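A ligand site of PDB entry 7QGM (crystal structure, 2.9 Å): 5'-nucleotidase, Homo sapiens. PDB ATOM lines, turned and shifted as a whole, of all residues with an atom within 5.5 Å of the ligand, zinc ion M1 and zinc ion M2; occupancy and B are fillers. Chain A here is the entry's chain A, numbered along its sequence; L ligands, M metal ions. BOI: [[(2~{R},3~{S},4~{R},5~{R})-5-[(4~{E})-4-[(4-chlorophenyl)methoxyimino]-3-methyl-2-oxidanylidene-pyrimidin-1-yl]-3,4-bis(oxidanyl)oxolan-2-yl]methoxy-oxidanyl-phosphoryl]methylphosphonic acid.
Zinc ion M2 is bound by O2 of the ligand (1.8 Å), OD1 of Asn 117 (2.1 Å), NE2 of His 220 (2.3 Å), ND1 of His 243 (2.3 Å) and OD2 of Asp 85 (2.4 Å).
Zinc ion M2 has five donor atoms within binding distance.
Slightly farther from zinc ion M2 lies OD1 of Asp 85 (2.8 Å).
Residues that only touch zinc ion M1: Asp 36 (3.3 Å) and Asn 245 (3.3 Å).
Within 4 Å of zinc ion M1: Asp 36, His 38, Asp 85 and Asn 245.
The nearest printed residue that does not touch zinc ion M1 is His 243 (4.7 Å).
The backbone NH of His 243 lies within hydrogen-bond range of the side-chain carboxylate of Asp 36.
OD1 of Asp 85 lies close to N of His 118 (3.3 Å).
The backbone carbonyl oxygen (O) of Gln 88 sits close to the backbone carbonyl oxygen (O) of His 38, 2.7 Å away.
The guanidinium group (NE) of Arg 395 lies within hydrogen-bond range of the backbone carbonyl oxygen (O) of Gly 392.
The side-chain amide nitrogen of Asn 390 sits close to the backbone NH of Gly 393, 3.0 Å away.
O of Gly 447 sits at hydrogen-bond distance from N of Gly 392 (2.8 Å).
The side-chain carboxylate (OD2) of Asp 36 lies close to the side-chain amide oxygen (OD1) of Asn 245 (3.2 Å).
The side-chain hydroxyl (OG) of Ser 185 lies within hydrogen-bond range of the side-chain carboxylate (OD1) of Asp 121.
O of Leu 184 lies close to O7 of the ligand (3.3 Å).
Merely in contact with the ligand: Gly 392, Gly 393, Asp 121, Gln 88, Phe 417, Asn 186, Phe 500 and Asn 245.
Hydrophobic or aromatic side chains that line the ligand: His 38, His 118, Leu 184, His 243, Phe 417 and Phe 500.
Of the 28 residues printed, 19 come within 4 Å of the ligand.
The nearest printed residue that does not touch the ligand is His 220 (4.1 Å).
His 118 touches zinc ion M2 (CD2 to ZN, 3.8 Å).
Within 4 Å of zinc ion M2: Asp 85, Asn 117, His 118, His 220 and His 243.
The nearest printed residue that does not touch zinc ion M2 is Asp 36 (4.7 Å).
Zinc ion M1 is bound by OD2 of Asp 85 and NE2 of His 38.
OD2 of Asp 506 lies within hydrogen-bond range of O9 of the ligand (2.6 Å).
The guanidinium group (NH1) of Arg 395 is in salt-bridge range of an oxygen (O) of the ligand (2.8 Å).
O9 of the ligand is in hydrogen-bond range of ND2 of Asn 390 (2.8 Å).
An oxygen (O1) of the ligand is in hydrogen-bond range of a ring nitrogen (NE2) of His 118 (3.0 Å).
The backbone carbonyl oxygen (O) of Gly 447 lies within hydrogen-bond range of an oxygen (O9) of the ligand, 3.1 Å away.
NH1 of Arg 354 lies within salt-bridge range of O3 of the ligand (3.4 Å).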
ATOM      1  N   ASP A  36      -2.068  27.985 -22.072  1.00  0.00           N
ATOM      2  CA  ASP A  36      -3.258  27.849 -22.907  1.00  0.00           C
ATOM      3  C   ASP A  36      -2.882  27.415 -24.330  1.00  0.00           C
ATOM      4  O   ASP A  36      -3.323  28.011 -25.315  1.00  0.00           O
ATOM      5  CB  ASP A  36      -4.060  29.150 -22.925  1.00  0.00           C
ATOM      6  CG  ASP A  36      -4.230  29.738 -21.534  1.00  0.00           C
ATOM      7  OD1 ASP A  36      -4.641  28.995 -20.610  1.00  0.00           O
ATOM      8  OD2 ASP A  36      -3.952  30.948 -21.357  1.00  0.00           O
ATOM      9  N   HIS A  38      -3.618  24.359 -25.564  1.00  0.00           N
ATOM     10  CA  HIS A  38      -4.803  23.633 -26.027  1.00  0.00           C
ATOM     11  C   HIS A  38      -4.457  22.694 -27.189  1.00  0.00           C
ATOM     12  O   HIS A  38      -5.114  22.697 -28.231  1.00  0.00           O
ATOM     13  CB  HIS A  38      -5.920  24.595 -26.397  1.00  0.00           C
ATOM     14  CG  HIS A  38      -6.530  25.290 -25.215  1.00  0.00           C
ATOM     15  ND1 HIS A  38      -7.108  24.599 -24.162  1.00  0.00           N
ATOM     16  CD2 HIS A  38      -6.659  26.606 -24.913  1.00  0.00           C
ATOM     17  CE1 HIS A  38      -7.555  25.465 -23.270  1.00  0.00           C
ATOM     18  NE2 HIS A  38      -7.293  26.683 -23.702  1.00  0.00           N
ATOM     19  N   ASP A  85      -3.688  24.573 -19.059  1.00  0.00           N
ATOM     20  CA  ASP A  85      -4.457  24.457 -20.297  1.00  0.00           C
ATOM     21  C   ASP A  85      -3.595  23.982 -21.466  1.00  0.00           C
ATOM     22  O   ASP A  85      -3.302  24.705 -22.410  1.00  0.00           O
ATOM     23  CB  ASP A  85      -5.142  25.786 -20.643  1.00  0.00           C
ATOM     24  CG  ASP A  85      -6.583  25.862 -20.169  1.00  0.00           C
ATOM     25  OD1 ASP A  85      -6.991  25.036 -19.315  1.00  0.00           O
ATOM     26  OD2 ASP A  85      -7.316  26.758 -20.637  1.00  0.00           O
ATOM     27  N   GLN A  88      -7.387  19.610 -24.568  1.00  0.00           N
ATOM     28  CA  GLN A  88      -8.465  20.044 -25.446  1.00  0.00           C
ATOM     29  C   GLN A  88      -7.957  20.941 -26.572  1.00  0.00           C
ATOM     30  O   GLN A  88      -6.735  21.031 -26.801  1.00  0.00           O
ATOM     31  CB  GLN A  88      -9.552  20.773 -24.653  1.00  0.00           C
ATOM     32  CG  GLN A  88     -10.682  19.851 -24.184  1.00  0.00           C
ATOM     33  CD  GLN A  88     -11.991  20.592 -24.028  1.00  0.00           C
ATOM     34  OE1 GLN A  88     -12.075  21.793 -24.259  1.00  0.00           O
ATOM     35  NE2 GLN A  88     -13.046  19.867 -23.642  1.00  0.00           N
ATOM     36  N   ASN A 117      -7.592  23.987 -15.653  1.00  0.00           N
ATOM     37  CA  ASN A 117      -8.938  23.457 -15.521  1.00  0.00           C
ATOM     38  C   ASN A 117      -9.237  22.423 -16.592  1.00  0.00           C
ATOM     39  O   ASN A 117      -9.998  21.477 -16.350  1.00  0.00           O
ATOM     40  CB  ASN A 117      -9.961  24.587 -15.562  1.00  0.00           C
ATOM     41  CG  ASN A 117     -10.296  25.030 -16.970  1.00  0.00           C
ATOM     42  OD1 ASN A 117      -9.553  25.781 -17.592  1.00  0.00           O
ATOM     43  ND2 ASN A 117     -11.439  24.557 -17.476  1.00  0.00           N
ATOM     44  N   HIS A 118      -8.650  22.566 -17.779  1.00  0.00           N
ATOM     45  CA  HIS A 118      -8.893  21.632 -18.874  1.00  0.00           C
ATOM     46  C   HIS A 118      -8.199  20.297 -18.700  1.00  0.00           C
ATOM     47  O   HIS A 118      -8.512  19.351 -19.429  1.00  0.00           O
ATOM     48  CB  HIS A 118      -8.477  22.257 -20.207  1.00  0.00           C
ATOM     49  CG  HIS A 118      -9.524  23.137 -20.817  1.00  0.00           C
ATOM     50  ND1 HIS A 118     -10.104  22.869 -22.036  1.00  0.00           N
ATOM     51  CD2 HIS A 118     -10.107  24.269 -20.365  1.00  0.00           C
ATOM     52  CE1 HIS A 118     -10.991  23.802 -22.323  1.00  0.00           C
ATOM     53  NE2 HIS A 118     -11.016  24.665 -21.316  1.00  0.00           N
ATOM     54  N   ASP A 121     -10.882  17.624 -18.085  1.00  0.00           N
ATOM     55  CA  ASP A 121     -11.991  17.416 -19.024  1.00  0.00           C
ATOM     56  C   ASP A 121     -12.184  15.942 -19.333  1.00  0.00           C
ATOM     57  O   ASP A 121     -13.301  15.520 -19.663  1.00  0.00           O
ATOM     58  CB  ASP A 121     -11.745  18.203 -20.310  1.00  0.00           C
ATOM     59  CG  ASP A 121     -11.738  19.705 -20.096  1.00  0.00           C
ATOM     60  OD1 ASP A 121     -12.286  20.177 -19.080  1.00  0.00           O
ATOM     61  OD2 ASP A 121     -11.175  20.423 -20.946  1.00  0.00           O
ATOM     62  N   ASN A 122     -11.126  15.137 -19.236  1.00  0.00           N
ATOM     63  CA  ASN A 122     -11.225  13.695 -19.408  1.00  0.00           C
ATOM     64  C   ASN A 122     -11.319  12.965 -18.077  1.00  0.00           C
ATOM     65  O   ASN A 122     -11.308  11.728 -18.058  1.00  0.00           O
ATOM     66  CB  ASN A 122     -10.052  13.176 -20.223  1.00  0.00           C
ATOM     67  CG  ASN A 122     -10.402  12.944 -21.683  1.00  0.00           C
ATOM     68  OD1 ASN A 122     -10.257  11.839 -22.201  1.00  0.00           O
ATOM     69  ND2 ASN A 122     -10.895  13.988 -22.339  1.00  0.00           N
ATOM     70  N   LEU A 184     -16.352  24.189 -14.042  1.00  0.00           N
ATOM     71  CA  LEU A 184     -15.908  24.400 -15.429  1.00  0.00           C
ATOM     72  C   LEU A 184     -15.431  23.127 -16.107  1.00  0.00           C
ATOM     73  O   LEU A 184     -15.355  23.099 -17.338  1.00  0.00           O
ATOM     74  CB  LEU A 184     -14.776  25.432 -15.462  1.00  0.00           C
ATOM     75  CG  LEU A 184     -14.968  26.654 -16.343  1.00  0.00           C
ATOM     76  CD1 LEU A 184     -14.227  27.852 -15.752  1.00  0.00           C
ATOM     77  CD2 LEU A 184     -14.490  26.371 -17.764  1.00  0.00           C
ATOM     78  N   SER A 185     -15.088  22.076 -15.361  1.00  0.00           N
ATOM     79  CA  SER A 185     -14.482  20.875 -15.915  1.00  0.00           C
ATOM     80  C   SER A 185     -15.107  19.680 -15.189  1.00  0.00           C
ATOM     81  O   SER A 185     -16.164  19.806 -14.552  1.00  0.00           O
ATOM     82  CB  SER A 185     -12.956  20.927 -15.780  1.00  0.00           C
ATOM     83  OG  SER A 185     -12.339  19.858 -16.474  1.00  0.00           O
ATOM     84  N   ASN A 186     -14.465  18.521 -15.277  1.00  0.00           N
ATOM     85  CA  ASN A 186     -14.948  17.284 -14.655  1.00  0.00           C
ATOM     86  C   ASN A 186     -13.853  16.685 -13.784  1.00  0.00           C
ATOM     87  O   ASN A 186     -13.250  15.662 -14.140  1.00  0.00           O
ATOM     88  CB  ASN A 186     -15.406  16.279 -15.713  1.00  0.00           C
ATOM     89  CG  ASN A 186     -16.083  16.922 -16.903  1.00  0.00           C
ATOM     90  OD1 ASN A 186     -17.057  17.669 -16.758  1.00  0.00           O
ATOM     91  ND2 ASN A 186     -15.575  16.644 -18.102  1.00  0.00           N
ATOM     92  N   HIS A 220      -3.231  28.859 -12.837  1.00  0.00           N
ATOM     93  CA  HIS A 220      -4.239  28.905 -13.894  1.00  0.00           C
ATOM     94  C   HIS A 220      -5.532  29.444 -13.285  1.00  0.00           C
ATOM     95  O   HIS A 220      -6.448  28.679 -12.978  1.00  0.00           O
ATOM     96  CB  HIS A 220      -4.420  27.516 -14.486  1.00  0.00           C
ATOM     97  CG  HIS A 220      -5.216  27.477 -15.747  1.00  0.00           C
ATOM     98  ND1 HIS A 220      -4.677  27.826 -16.966  1.00  0.00           N
ATOM     99  CD2 HIS A 220      -6.503  27.119 -15.983  1.00  0.00           C
ATOM    100  CE1 HIS A 220      -5.608  27.693 -17.900  1.00  0.00           C
ATOM    101  NE2 HIS A 220      -6.722  27.269 -17.326  1.00  0.00           N
ATOM    102  N   HIS A 243      -5.036  31.207 -18.085  1.00  0.00           N
ATOM    103  CA  HIS A 243      -6.448  30.846 -18.075  1.00  0.00           C
ATOM    104  C   HIS A 243      -7.376  31.925 -18.628  1.00  0.00           C
ATOM    105  O   HIS A 243      -8.526  31.612 -18.947  1.00  0.00           O
ATOM    106  CB  HIS A 243      -6.976  30.488 -16.663  1.00  0.00           C
ATOM    107  CG  HIS A 243      -8.432  30.147 -16.636  1.00  0.00           C
ATOM    108  ND1 HIS A 243      -8.927  29.012 -17.221  1.00  0.00           N
ATOM    109  CD2 HIS A 243      -9.495  30.802 -16.121  1.00  0.00           C
ATOM    110  CE1 HIS A 243     -10.237  28.963 -17.054  1.00  0.00           C
ATOM    111  NE2 HIS A 243     -10.612  30.042 -16.392  1.00  0.00           N
ATOM    112  N   ASN A 245      -6.045  33.909 -21.263  1.00  0.00           N
ATOM    113  CA  ASN A 245      -5.410  34.146 -22.557  1.00  0.00           C
ATOM    114  C   ASN A 245      -5.137  35.636 -22.744  1.00  0.00           C
ATOM    115  O   ASN A 245      -5.621  36.282 -23.672  1.00  0.00           O
ATOM    116  CB  ASN A 245      -6.264  33.578 -23.685  1.00  0.00           C
ATOM    117  CG  ASN A 245      -6.853  32.209 -23.347  1.00  0.00           C
ATOM    118  OD1 ASN A 245      -6.215  31.172 -23.550  1.00  0.00           O
ATOM    119  ND2 ASN A 245      -8.070  32.205 -22.828  1.00  0.00           N
ATOM    120  N   ARG A 354     -17.700  36.631 -28.805  1.00  0.00           N
ATOM    121  CA  ARG A 354     -18.067  37.059 -27.455  1.00  0.00           C
ATOM    122  C   ARG A 354     -18.298  38.567 -27.389  1.00  0.00           C
ATOM    123  O   ARG A 354     -18.437  39.107 -26.286  1.00  0.00           O
ATOM    124  CB  ARG A 354     -16.989  36.638 -26.458  1.00  0.00           C
ATOM    125  CG  ARG A 354     -16.809  35.127 -26.344  1.00  0.00           C
ATOM    126  CD  ARG A 354     -15.376  34.758 -25.967  1.00  0.00           C
ATOM    127  NE  ARG A 354     -15.118  33.331 -26.108  1.00  0.00           N
ATOM    128  CZ  ARG A 354     -14.616  32.558 -25.146  1.00  0.00           C
ATOM    129  NH1 ARG A 354     -14.267  33.053 -23.966  1.00  0.00           N
ATOM    130  NH2 ARG A 354     -14.436  31.263 -25.394  1.00  0.00           N
ATOM    131  N   ASN A 390     -23.982  29.961 -26.385  1.00  0.00           N
ATOM    132  CA  ASN A 390     -22.939  30.728 -25.720  1.00  0.00           C
ATOM    133  C   ASN A 390     -21.702  30.770 -26.600  1.00  0.00           C
ATOM    134  O   ASN A 390     -21.131  29.722 -26.925  1.00  0.00           O
ATOM    135  CB  ASN A 390     -22.617  30.135 -24.345  1.00  0.00           C
ATOM    136  CG  ASN A 390     -22.067  28.706 -24.427  1.00  0.00           C
ATOM    137  OD1 ASN A 390     -22.801  27.765 -24.731  1.00  0.00           O
ATOM    138  ND2 ASN A 390     -20.788  28.552 -24.120  1.00  0.00           N
ATOM    139  N   GLY A 391     -21.264  31.973 -26.977  1.00  0.00           N
ATOM    140  CA  GLY A 391     -20.096  32.102 -27.827  1.00  0.00           C
ATOM    141  C   GLY A 391     -18.860  31.450 -27.253  1.00  0.00           C
ATOM    142  O   GLY A 391     -17.945  31.100 -28.010  1.00  0.00           O
ATOM    143  N   GLY A 392     -18.817  31.272 -25.932  1.00  0.00           N
ATOM    144  CA  GLY A 392     -17.694  30.585 -25.330  1.00  0.00           C
ATOM    145  C   GLY A 392     -17.535  29.162 -25.809  1.00  0.00           C
ATOM    146  O   GLY A 392     -16.407  28.643 -25.874  1.00  0.00           O
ATOM    147  N   GLY A 393     -18.635  28.493 -26.156  1.00  0.00           N
ATOM    148  CA  GLY A 393     -18.538  27.150 -26.678  1.00  0.00           C
ATOM    149  C   GLY A 393     -17.803  27.080 -27.997  1.00  0.00           C
ATOM    150  O   GLY A 393     -17.206  26.047 -28.325  1.00  0.00           O
ATOM    151  N   ARG A 395     -14.816  27.526 -30.098  1.00  0.00           N
ATOM    152  CA  ARG A 395     -13.433  27.567 -29.669  1.00  0.00           C
ATOM    153  C   ARG A 395     -12.424  27.684 -30.801  1.00  0.00           C
ATOM    154  O   ARG A 395     -11.217  27.784 -30.522  1.00  0.00           O
ATOM    155  CB  ARG A 395     -13.104  26.322 -28.824  1.00  0.00           C
ATOM    156  CG  ARG A 395     -13.752  26.310 -27.445  1.00  0.00           C
ATOM    157  CD  ARG A 395     -13.411  27.574 -26.667  1.00  0.00           C
ATOM    158  NE  ARG A 395     -13.875  27.523 -25.288  1.00  0.00           N
ATOM    159  CZ  ARG A 395     -13.151  27.090 -24.269  1.00  0.00           C
ATOM    160  NH1 ARG A 395     -11.925  26.607 -24.434  1.00  0.00           N
ATOM    161  NH2 ARG A 395     -13.670  27.124 -23.041  1.00  0.00           N
ATOM    162  N   PRO A 416     -14.727  21.325 -28.943  1.00  0.00           N
ATOM    163  CA  PRO A 416     -13.981  20.269 -28.244  1.00  0.00           C
ATOM    164  C   PRO A 416     -14.761  19.569 -27.148  1.00  0.00           C
ATOM    165  O   PRO A 416     -14.342  18.490 -26.703  1.00  0.00           O
ATOM    166  CB  PRO A 416     -12.768  21.015 -27.668  1.00  0.00           C
ATOM    167  CG  PRO A 416     -13.275  22.421 -27.467  1.00  0.00           C
ATOM    168  CD  PRO A 416     -14.220  22.678 -28.624  1.00  0.00           C
ATOM    169  N   PHE A 417     -15.882  20.143 -26.703  1.00  0.00           N
ATOM    170  CA  PHE A 417     -16.554  19.618 -25.515  1.00  0.00           C
ATOM    171  C   PHE A 417     -17.323  18.341 -25.818  1.00  0.00           C
ATOM    172  O   PHE A 417     -17.393  17.436 -24.972  1.00  0.00           O
ATOM    173  CB  PHE A 417     -17.491  20.686 -24.950  1.00  0.00           C
ATOM    174  CG  PHE A 417     -16.836  22.023 -24.782  1.00  0.00           C
ATOM    175  CD1 PHE A 417     -16.150  22.334 -23.617  1.00  0.00           C
ATOM    176  CD2 PHE A 417     -16.902  22.973 -25.784  1.00  0.00           C
ATOM    177  CE1 PHE A 417     -15.551  23.573 -23.462  1.00  0.00           C
ATOM    178  CE2 PHE A 417     -16.303  24.212 -25.630  1.00  0.00           C
ATOM    179  CZ  PHE A 417     -15.630  24.510 -24.465  1.00  0.00           C
ATOM    180  N   SER A 445     -14.165  39.760 -22.632  1.00  0.00           N
ATOM    181  CA  SER A 445     -14.025  38.527 -23.407  1.00  0.00           C
ATOM    182  C   SER A 445     -14.884  37.418 -22.807  1.00  0.00           C
ATOM    183  O   SER A 445     -14.546  36.230 -22.898  1.00  0.00           O
ATOM    184  CB  SER A 445     -12.562  38.098 -23.512  1.00  0.00           C
ATOM    185  OG  SER A 445     -12.385  37.089 -24.497  1.00  0.00           O
ATOM    186  N   THR A 446     -16.000  37.810 -22.196  1.00  0.00           N
ATOM    187  CA  THR A 446     -16.812  36.894 -21.422  1.00  0.00           C
ATOM    188  C   THR A 446     -17.458  35.855 -22.326  1.00  0.00           C
ATOM    189  O   THR A 446     -18.056  36.200 -23.352  1.00  0.00           O
ATOM    190  CB  THR A 446     -17.868  37.667 -20.654  1.00  0.00           C
ATOM    191  OG1 THR A 446     -18.625  38.467 -21.578  1.00  0.00           O
ATOM    192  CG2 THR A 446     -17.214  38.580 -19.622  1.00  0.00           C
ATOM    193  N   GLY A 447     -17.359  34.591 -21.935  1.00  0.00           N
ATOM    194  CA  GLY A 447     -17.824  33.497 -22.760  1.00  0.00           C
ATOM    195  C   GLY A 447     -19.320  33.246 -22.733  1.00  0.00           C
ATOM    196  O   GLY A 447     -19.802  32.456 -23.554  1.00  0.00           O
ATOM    197  N   GLU A 448     -20.063  33.902 -21.839  1.00  0.00           N
ATOM    198  CA  GLU A 448     -21.495  33.700 -21.739  1.00  0.00           C
ATOM    199  C   GLU A 448     -22.290  34.573 -22.707  1.00  0.00           C
ATOM    200  O   GLU A 448     -23.523  34.565 -22.664  1.00  0.00           O
ATOM    201  CB  GLU A 448     -21.971  33.931 -20.288  1.00  0.00           C
ATOM    202  CG  GLU A 448     -22.143  35.385 -19.843  1.00  0.00           C
ATOM    203  CD  GLU A 448     -20.841  36.054 -19.481  1.00  0.00           C
ATOM    204  OE1 GLU A 448     -19.829  35.343 -19.298  1.00  0.00           O
ATOM    205  OE2 GLU A 448     -20.826  37.303 -19.366  1.00  0.00           O
ATOM    206  N   PHE A 500     -24.886  22.103 -22.132  1.00  0.00           N
ATOM    207  CA  PHE A 500     -24.215  22.918 -21.117  1.00  0.00           C
ATOM    208  C   PHE A 500     -25.076  24.127 -20.721  1.00  0.00           C
ATOM    209  O   PHE A 500     -25.091  24.522 -19.550  1.00  0.00           O
ATOM    210  CB  PHE A 500     -22.840  23.337 -21.640  1.00  0.00           C
ATOM    211  CG  PHE A 500     -22.240  24.520 -20.932  1.00  0.00           C
ATOM    212  CD1 PHE A 500     -21.767  24.409 -19.637  1.00  0.00           C
ATOM    213  CD2 PHE A 500     -22.135  25.739 -21.588  1.00  0.00           C
ATOM    214  CE1 PHE A 500     -21.224  25.512 -18.998  1.00  0.00           C
ATOM    215  CE2 PHE A 500     -21.592  26.833 -20.953  1.00  0.00           C
ATOM    216  CZ  PHE A 500     -21.132  26.719 -19.655  1.00  0.00           C
ATOM    217  N   ASP A 506     -22.621  28.692 -17.169  1.00  0.00           N
ATOM    218  CA  ASP A 506     -22.111  30.041 -17.415  1.00  0.00           C
ATOM    219  C   ASP A 506     -22.798  31.102 -16.568  1.00  0.00           C
ATOM    220  O   ASP A 506     -22.558  32.296 -16.773  1.00  0.00           O
ATOM    221  CB  ASP A 506     -22.242  30.409 -18.900  1.00  0.00           C
ATOM    222  CG  ASP A 506     -20.909  30.637 -19.567  1.00  0.00           C
ATOM    223  OD1 ASP A 506     -19.945  30.998 -18.857  1.00  0.00           O
ATOM    224  OD2 ASP A 506     -20.823  30.450 -20.794  1.00  0.00           O
HETATM  225  O8  BOI L   1     -18.954  25.951 -23.513  1.00  0.00           O
HETATM  226  C15 BOI L   1     -18.451  25.577 -22.471  1.00  0.00           C
HETATM  227  N2  BOI L   1     -18.643  24.287 -21.988  1.00  0.00           N
HETATM  228  C14 BOI L   1     -19.427  23.377 -22.825  1.00  0.00           C
HETATM  229  C6  BOI L   1     -18.159  23.821 -20.771  1.00  0.00           C
HETATM  230  N1  BOI L   1     -18.464  22.601 -20.480  1.00  0.00           N
HETATM  231  O7  BOI L   1     -17.928  22.213 -19.223  1.00  0.00           O
HETATM  232  C7  BOI L   1     -18.298  20.846 -18.996  1.00  0.00           C
HETATM  233  C8  BOI L   1     -17.451  19.926 -19.821  1.00  0.00           C
HETATM  234  C13 BOI L   1     -16.057  20.034 -19.809  1.00  0.00           C
HETATM  235  C12 BOI L   1     -15.275  19.202 -20.575  1.00  0.00           C
HETATM  236  C11 BOI L   1     -15.870  18.247 -21.362  1.00  0.00           C
HETATM  237 CL   BOI L   1     -14.886  17.208 -22.349  1.00  0.00          CL
HETATM  238  C10 BOI L   1     -17.240  18.108 -21.396  1.00  0.00           C
HETATM  239  C9  BOI L   1     -18.024  18.949 -20.627  1.00  0.00           C
HETATM  240  C5  BOI L   1     -17.391  24.741 -20.002  1.00  0.00           C
HETATM  241  C4  BOI L   1     -17.191  25.982 -20.464  1.00  0.00           C
HETATM  242  N   BOI L   1     -17.687  26.410 -21.667  1.00  0.00           N
HETATM  243  C3  BOI L   1     -17.444  27.780 -22.148  1.00  0.00           C
HETATM  244  O6  BOI L   1     -16.076  28.090 -21.955  1.00  0.00           O
HETATM  245  C16 BOI L   1     -18.270  28.846 -21.400  1.00  0.00           C
HETATM  246  O9  BOI L   1     -18.915  29.690 -22.348  1.00  0.00           O
HETATM  247  C17 BOI L   1     -17.215  29.613 -20.601  1.00  0.00           C
HETATM  248  O10 BOI L   1     -17.534  30.994 -20.442  1.00  0.00           O
HETATM  249  C2  BOI L   1     -15.963  29.435 -21.450  1.00  0.00           C
HETATM  250  C1  BOI L   1     -14.657  29.612 -20.725  1.00  0.00           C
HETATM  251  O5  BOI L   1     -13.590  29.748 -21.699  1.00  0.00           O
HETATM  252  P1  BOI L   1     -12.366  30.705 -21.468  1.00  0.00           P
HETATM  253  O3  BOI L   1     -12.761  32.089 -21.029  1.00  0.00           O
HETATM  254  O4  BOI L   1     -11.661  30.832 -22.850  1.00  0.00           O
HETATM  255  C   BOI L   1     -11.251  29.751 -20.418  1.00  0.00           C
HETATM  256  P   BOI L   1     -10.942  28.043 -20.906  1.00  0.00           P
HETATM  257  O   BOI L   1     -10.583  27.889 -22.349  1.00  0.00           O
HETATM  258  O2  BOI L   1      -9.833  27.510 -19.974  1.00  0.00           O
HETATM  259  O1  BOI L   1     -12.229  27.275 -20.548  1.00  0.00           O
HETATM  260 ZN    ZN M   1      -7.479  28.437 -22.212  1.00  0.00          ZN
HETATM  261 ZN    ZN M   2      -8.552  27.304 -18.709  1.00  0.00          ZN
